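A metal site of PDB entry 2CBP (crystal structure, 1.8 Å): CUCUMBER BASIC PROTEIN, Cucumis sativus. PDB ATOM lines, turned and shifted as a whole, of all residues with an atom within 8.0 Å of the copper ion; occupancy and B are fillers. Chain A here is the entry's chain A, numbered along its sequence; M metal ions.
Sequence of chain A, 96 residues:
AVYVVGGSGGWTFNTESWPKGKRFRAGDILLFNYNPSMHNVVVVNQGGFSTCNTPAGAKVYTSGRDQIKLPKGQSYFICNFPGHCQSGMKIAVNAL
The copper ion is bound by a ring nitrogen (ND1) of His 39 (1.9 Å), a ring nitrogen (ND1) of His 84 (2.0 Å), the side-chain sulfur (SG) of Cys 79 (2.1 Å) and the side-chain sulfur (SD) of Met 89 (2.6 Å).
O of Cys 79 sits at hydrogen-bond distance from N of Cys 85 (3.4 Å).
The backbone NH (N) of Phe 81 lies close to the side-chain sulfur (SG) of Cys 79, at 3.8 Å.
SG of Cys 79 lies close to OD1 of Asn 40, at 3.6 Å.
Merely in contact with the copper ion: Met 38 (3.8 Å).
Five residues have an atom within 4 Å of the copper ion: Met 38, His 39, Cys 79, His 84 and Met 89.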
ATOM      1  N   TRP A  11     -10.415   2.961  11.178  1.00  0.00           N
ATOM      2  CA  TRP A  11     -10.702   1.511  11.030  1.00  0.00           C
ATOM      3  C   TRP A  11      -9.517   0.927  10.257  1.00  0.00           C
ATOM      4  O   TRP A  11      -9.361   1.226   9.086  1.00  0.00           O
ATOM      5  CB  TRP A  11     -12.046   1.315  10.401  1.00  0.00           C
ATOM      6  CG  TRP A  11     -12.564  -0.034  10.067  1.00  0.00           C
ATOM      7  CD1 TRP A  11     -13.051  -0.434   8.868  1.00  0.00           C
ATOM      8  CD2 TRP A  11     -12.701  -1.159  10.944  1.00  0.00           C
ATOM      9  NE1 TRP A  11     -13.514  -1.747   8.908  1.00  0.00           N
ATOM     10  CE2 TRP A  11     -13.296  -2.208  10.196  1.00  0.00           C
ATOM     11  CE3 TRP A  11     -12.407  -1.363  12.284  1.00  0.00           C
ATOM     12  CZ2 TRP A  11     -13.571  -3.446  10.744  1.00  0.00           C
ATOM     13  CZ3 TRP A  11     -12.685  -2.604  12.840  1.00  0.00           C
ATOM     14  CH2 TRP A  11     -13.248  -3.630  12.078  1.00  0.00           C
ATOM     15  N   THR A  12      -8.737   0.152  10.992  1.00  0.00           N
ATOM     16  CA  THR A  12      -7.515  -0.441  10.396  1.00  0.00           C
ATOM     17  C   THR A  12      -7.139  -1.736  11.060  1.00  0.00           C
ATOM     18  O   THR A  12      -7.891  -2.283  11.884  1.00  0.00           O
ATOM     19  CB  THR A  12      -6.454   0.664  10.500  1.00  0.00           C
ATOM     20  OG1 THR A  12      -5.375   0.226   9.711  1.00  0.00           O
ATOM     21  CG2 THR A  12      -6.037   0.961  11.939  1.00  0.00           C
ATOM     22  N   PHE A  13      -5.965  -2.241  10.708  1.00  0.00           N
ATOM     23  CA  PHE A  13      -5.400  -3.495  11.216  1.00  0.00           C
ATOM     24  C   PHE A  13      -5.061  -3.454  12.706  1.00  0.00           C
ATOM     25  O   PHE A  13      -4.847  -2.384  13.281  1.00  0.00           O
ATOM     26  CB  PHE A  13      -4.148  -3.873  10.410  1.00  0.00           C
ATOM     27  CG  PHE A  13      -4.360  -4.021   8.927  1.00  0.00           C
ATOM     28  CD1 PHE A  13      -4.873  -5.199   8.402  1.00  0.00           C
ATOM     29  CD2 PHE A  13      -4.015  -2.969   8.060  1.00  0.00           C
ATOM     30  CE1 PHE A  13      -5.065  -5.346   7.027  1.00  0.00           C
ATOM     31  CE2 PHE A  13      -4.202  -3.099   6.684  1.00  0.00           C
ATOM     32  CZ  PHE A  13      -4.738  -4.297   6.176  1.00  0.00           C
ATOM     33  N   TYR A  34     -12.414   4.861   6.724  1.00  0.00           N
ATOM     34  CA  TYR A  34     -11.435   4.072   5.946  1.00  0.00           C
ATOM     35  C   TYR A  34     -11.582   4.301   4.454  1.00  0.00           C
ATOM     36  O   TYR A  34     -12.565   4.899   3.979  1.00  0.00           O
ATOM     37  CB  TYR A  34     -11.672   2.543   6.264  1.00  0.00           C
ATOM     38  CG  TYR A  34     -13.081   2.202   5.902  1.00  0.00           C
ATOM     39  CD1 TYR A  34     -14.162   2.458   6.765  1.00  0.00           C
ATOM     40  CD2 TYR A  34     -13.389   1.624   4.645  1.00  0.00           C
ATOM     41  CE1 TYR A  34     -15.450   2.186   6.411  1.00  0.00           C
ATOM     42  CE2 TYR A  34     -14.690   1.357   4.290  1.00  0.00           C
ATOM     43  CZ  TYR A  34     -15.733   1.620   5.167  1.00  0.00           C
ATOM     44  OH  TYR A  34     -16.994   1.333   4.722  1.00  0.00           O
ATOM     45  N   ASN A  35     -10.619   3.748   3.738  1.00  0.00           N
ATOM     46  CA  ASN A  35     -10.583   3.771   2.255  1.00  0.00           C
ATOM     47  C   ASN A  35     -11.353   2.552   1.754  1.00  0.00           C
ATOM     48  O   ASN A  35     -10.780   1.460   1.873  1.00  0.00           O
ATOM     49  CB  ASN A  35      -9.119   3.687   1.805  1.00  0.00           C
ATOM     50  CG  ASN A  35      -9.006   3.769   0.280  1.00  0.00           C
ATOM     51  OD1 ASN A  35      -9.968   3.471  -0.452  1.00  0.00           O
ATOM     52  ND2 ASN A  35      -7.833   4.189  -0.181  1.00  0.00           N
ATOM     53  N   MET A  38      -9.976  -0.468  -0.117  1.00  0.00           N
ATOM     54  CA  MET A  38      -9.137  -1.376   0.617  1.00  0.00           C
ATOM     55  C   MET A  38      -9.716  -2.054   1.848  1.00  0.00           C
ATOM     56  O   MET A  38      -9.057  -2.960   2.385  1.00  0.00           O
ATOM     57  CB  MET A  38      -7.911  -0.525   1.160  1.00  0.00           C
ATOM     58  CG  MET A  38      -7.272   0.223   0.013  1.00  0.00           C
ATOM     59  SD  MET A  38      -5.644   0.859   0.392  1.00  0.00           S
ATOM     60  CE  MET A  38      -5.957   1.677   1.969  1.00  0.00           C
ATOM     61  N   HIS A  39     -10.854  -1.592   2.291  1.00  0.00           N
ATOM     62  CA  HIS A  39     -11.523  -2.124   3.498  1.00  0.00           C
ATOM     63  C   HIS A  39     -13.038  -1.959   3.436  1.00  0.00           C
ATOM     64  O   HIS A  39     -13.565  -1.209   2.645  1.00  0.00           O
ATOM     65  CB  HIS A  39     -10.992  -1.370   4.727  1.00  0.00           C
ATOM     66  CG  HIS A  39      -9.538  -1.393   5.033  1.00  0.00           C
ATOM     67  ND1 HIS A  39      -8.886  -2.512   5.582  1.00  0.00           N
ATOM     68  CD2 HIS A  39      -8.619  -0.389   4.880  1.00  0.00           C
ATOM     69  CE1 HIS A  39      -7.641  -2.157   5.701  1.00  0.00           C
ATOM     70  NE2 HIS A  39      -7.427  -0.896   5.307  1.00  0.00           N
ATOM     71  N   ASN A  40     -13.715  -2.678   4.336  1.00  0.00           N
ATOM     72  CA  ASN A  40     -15.158  -2.670   4.493  1.00  0.00           C
ATOM     73  C   ASN A  40     -15.447  -2.922   5.993  1.00  0.00           C
ATOM     74  O   ASN A  40     -14.545  -3.143   6.806  1.00  0.00           O
ATOM     75  CB  ASN A  40     -15.939  -3.654   3.600  1.00  0.00           C
ATOM     76  CG  ASN A  40     -15.560  -5.096   3.774  1.00  0.00           C
ATOM     77  OD1 ASN A  40     -15.005  -5.480   4.837  1.00  0.00           O
ATOM     78  ND2 ASN A  40     -15.785  -5.942   2.766  1.00  0.00           N
ATOM     79  N   VAL A  41     -16.746  -2.852   6.264  1.00  0.00           N
ATOM     80  CA  VAL A  41     -17.261  -3.102   7.635  1.00  0.00           C
ATOM     81  C   VAL A  41     -18.354  -4.159   7.430  1.00  0.00           C
ATOM     82  O   VAL A  41     -19.300  -3.925   6.645  1.00  0.00           O
ATOM     83  CB  VAL A  41     -17.761  -1.821   8.331  1.00  0.00           C
ATOM     84  CG1 VAL A  41     -18.366  -2.112   9.703  1.00  0.00           C
ATOM     85  CG2 VAL A  41     -16.714  -0.740   8.409  1.00  0.00           C
ATOM     86  N   ILE A  78     -16.229  -7.050  11.473  1.00  0.00           N
ATOM     87  CA  ILE A  78     -14.958  -7.489  10.906  1.00  0.00           C
ATOM     88  C   ILE A  78     -14.800  -6.798   9.521  1.00  0.00           C
ATOM     89  O   ILE A  78     -15.774  -6.253   9.001  1.00  0.00           O
ATOM     90  CB  ILE A  78     -14.849  -8.993  10.681  1.00  0.00           C
ATOM     91  CG1 ILE A  78     -15.796  -9.432   9.578  1.00  0.00           C
ATOM     92  CG2 ILE A  78     -15.102  -9.810  11.935  1.00  0.00           C
ATOM     93  CD1 ILE A  78     -15.761 -10.918   9.193  1.00  0.00           C
ATOM     94  N   CYS A  79     -13.586  -6.853   9.040  1.00  0.00           N
ATOM     95  CA  CYS A  79     -13.275  -6.364   7.670  1.00  0.00           C
ATOM     96  C   CYS A  79     -13.105  -7.722   6.938  1.00  0.00           C
ATOM     97  O   CYS A  79     -12.302  -8.511   7.491  1.00  0.00           O
ATOM     98  CB  CYS A  79     -12.068  -5.497   7.543  1.00  0.00           C
ATOM     99  SG  CYS A  79     -11.509  -5.272   5.831  1.00  0.00           S
ATOM    100  N   ASN A  80     -13.816  -7.970   5.864  1.00  0.00           N
ATOM    101  CA  ASN A  80     -13.669  -9.279   5.206  1.00  0.00           C
ATOM    102  C   ASN A  80     -12.796  -9.326   3.964  1.00  0.00           C
ATOM    103  O   ASN A  80     -12.829 -10.368   3.259  1.00  0.00           O
ATOM    104  CB  ASN A  80     -14.963 -10.058   5.113  1.00  0.00           C
ATOM    105  CG  ASN A  80     -15.886  -9.623   3.996  1.00  0.00           C
ATOM    106  OD1 ASN A  80     -15.552  -8.695   3.238  1.00  0.00           O
ATOM    107  ND2 ASN A  80     -17.008 -10.306   3.926  1.00  0.00           N
ATOM    108  N   PHE A  81     -11.994  -8.345   3.701  1.00  0.00           N
ATOM    109  CA  PHE A  81     -10.981  -8.347   2.621  1.00  0.00           C
ATOM    110  C   PHE A  81     -10.047  -9.497   3.038  1.00  0.00           C
ATOM    111  O   PHE A  81      -9.851  -9.773   4.225  1.00  0.00           O
ATOM    112  CB  PHE A  81     -10.233  -7.020   2.574  1.00  0.00           C
ATOM    113  CG  PHE A  81     -10.871  -5.990   1.679  1.00  0.00           C
ATOM    114  CD1 PHE A  81     -12.159  -5.536   1.896  1.00  0.00           C
ATOM    115  CD2 PHE A  81     -10.150  -5.483   0.612  1.00  0.00           C
ATOM    116  CE1 PHE A  81     -12.741  -4.570   1.043  1.00  0.00           C
ATOM    117  CE2 PHE A  81     -10.698  -4.530  -0.250  1.00  0.00           C
ATOM    118  CZ  PHE A  81     -11.976  -4.093  -0.038  1.00  0.00           C
ATOM    119  N   PRO A  82      -9.505 -10.216   2.083  1.00  0.00           N
ATOM    120  CA  PRO A  82      -8.639 -11.366   2.368  1.00  0.00           C
ATOM    121  C   PRO A  82      -7.527 -11.045   3.313  1.00  0.00           C
ATOM    122  O   PRO A  82      -6.679 -10.169   3.126  1.00  0.00           O
ATOM    123  CB  PRO A  82      -8.195 -11.870   0.998  1.00  0.00           C
ATOM    124  CG  PRO A  82      -9.273 -11.379   0.026  1.00  0.00           C
ATOM    125  CD  PRO A  82      -9.668 -10.002   0.614  1.00  0.00           C
ATOM    126  N   GLY A  83      -7.524 -11.819   4.417  1.00  0.00           N
ATOM    127  CA  GLY A  83      -6.533 -11.663   5.467  1.00  0.00           C
ATOM    128  C   GLY A  83      -6.691 -10.525   6.428  1.00  0.00           C
ATOM    129  O   GLY A  83      -5.871 -10.422   7.361  1.00  0.00           O
ATOM    130  N   HIS A  84      -7.689  -9.658   6.258  1.00  0.00           N
ATOM    131  CA  HIS A  84      -7.818  -8.508   7.199  1.00  0.00           C
ATOM    132  C   HIS A  84      -8.309  -8.926   8.576  1.00  0.00           C
ATOM    133  O   HIS A  84      -7.733  -8.444   9.564  1.00  0.00           O
ATOM    134  CB  HIS A  84      -8.673  -7.414   6.571  1.00  0.00           C
ATOM    135  CG  HIS A  84      -7.993  -6.700   5.420  1.00  0.00           C
ATOM    136  ND1 HIS A  84      -8.194  -5.365   5.198  1.00  0.00           N
ATOM    137  CD2 HIS A  84      -7.129  -7.180   4.471  1.00  0.00           C
ATOM    138  CE1 HIS A  84      -7.517  -5.053   4.129  1.00  0.00           C
ATOM    139  NE2 HIS A  84      -6.843  -6.106   3.655  1.00  0.00           N
ATOM    140  N   CYS A  85      -9.350  -9.764   8.580  1.00  0.00           N
ATOM    141  CA  CYS A  85      -9.915 -10.256   9.857  1.00  0.00           C
ATOM    142  C   CYS A  85      -8.828 -10.980  10.631  1.00  0.00           C
ATOM    143  O   CYS A  85      -8.643 -10.798  11.838  1.00  0.00           O
ATOM    144  CB  CYS A  85     -11.143 -11.111   9.597  1.00  0.00           C
ATOM    145  SG  CYS A  85     -11.936 -11.741  11.077  1.00  0.00           S
ATOM    146  N   SER A  87      -5.823 -10.496  10.528  1.00  0.00           N
ATOM    147  CA  SER A  87      -4.762  -9.572  10.946  1.00  0.00           C
ATOM    148  C   SER A  87      -5.230  -8.671  12.075  1.00  0.00           C
ATOM    149  O   SER A  87      -4.494  -7.701  12.381  1.00  0.00           O
ATOM    150  CB  SER A  87      -4.265  -8.720   9.775  1.00  0.00           C
ATOM    151  OG  SER A  87      -3.782  -9.512   8.713  1.00  0.00           O
ATOM    152  N   MET A  89      -8.345  -7.015  12.213  1.00  0.00           N
ATOM    153  CA  MET A  89      -9.281  -5.978  11.731  1.00  0.00           C
ATOM    154  C   MET A  89     -10.704  -6.476  12.041  1.00  0.00           C
ATOM    155  O   MET A  89     -11.462  -6.951  11.224  1.00  0.00           O
ATOM    156  CB  MET A  89      -9.026  -5.616  10.274  1.00  0.00           C
ATOM    157  CG  MET A  89      -9.820  -4.401   9.880  1.00  0.00           C
ATOM    158  SD  MET A  89      -9.100  -3.581   8.425  1.00  0.00           S
ATOM    159  CE  MET A  89     -10.293  -2.186   8.393  1.00  0.00           C
ATOM    160  N   LYS A  90     -10.969  -6.391  13.354  1.00  0.00           N
ATOM    161  CA  LYS A  90     -12.241  -6.821  13.931  1.00  0.00           C
ATOM    162  C   LYS A  90     -12.397  -6.255  15.341  1.00  0.00           C
ATOM    163  O   LYS A  90     -11.396  -5.991  16.023  1.00  0.00           O
ATOM    164  CB  LYS A  90     -12.284  -8.374  14.041  1.00  0.00           C
ATOM    165  CG  LYS A  90     -11.167  -8.865  14.933  1.00  0.00           C
ATOM    166  CD  LYS A  90     -11.245 -10.208  15.542  1.00  0.00           C
ATOM    167  CE  LYS A  90     -11.369 -11.378  14.648  1.00  0.00           C
ATOM    168  NZ  LYS A  90     -11.182 -12.656  15.440  1.00  0.00           N
HETATM  169 CU    CU M   1      -9.618  -4.257   5.959  1.00  0.00          CU
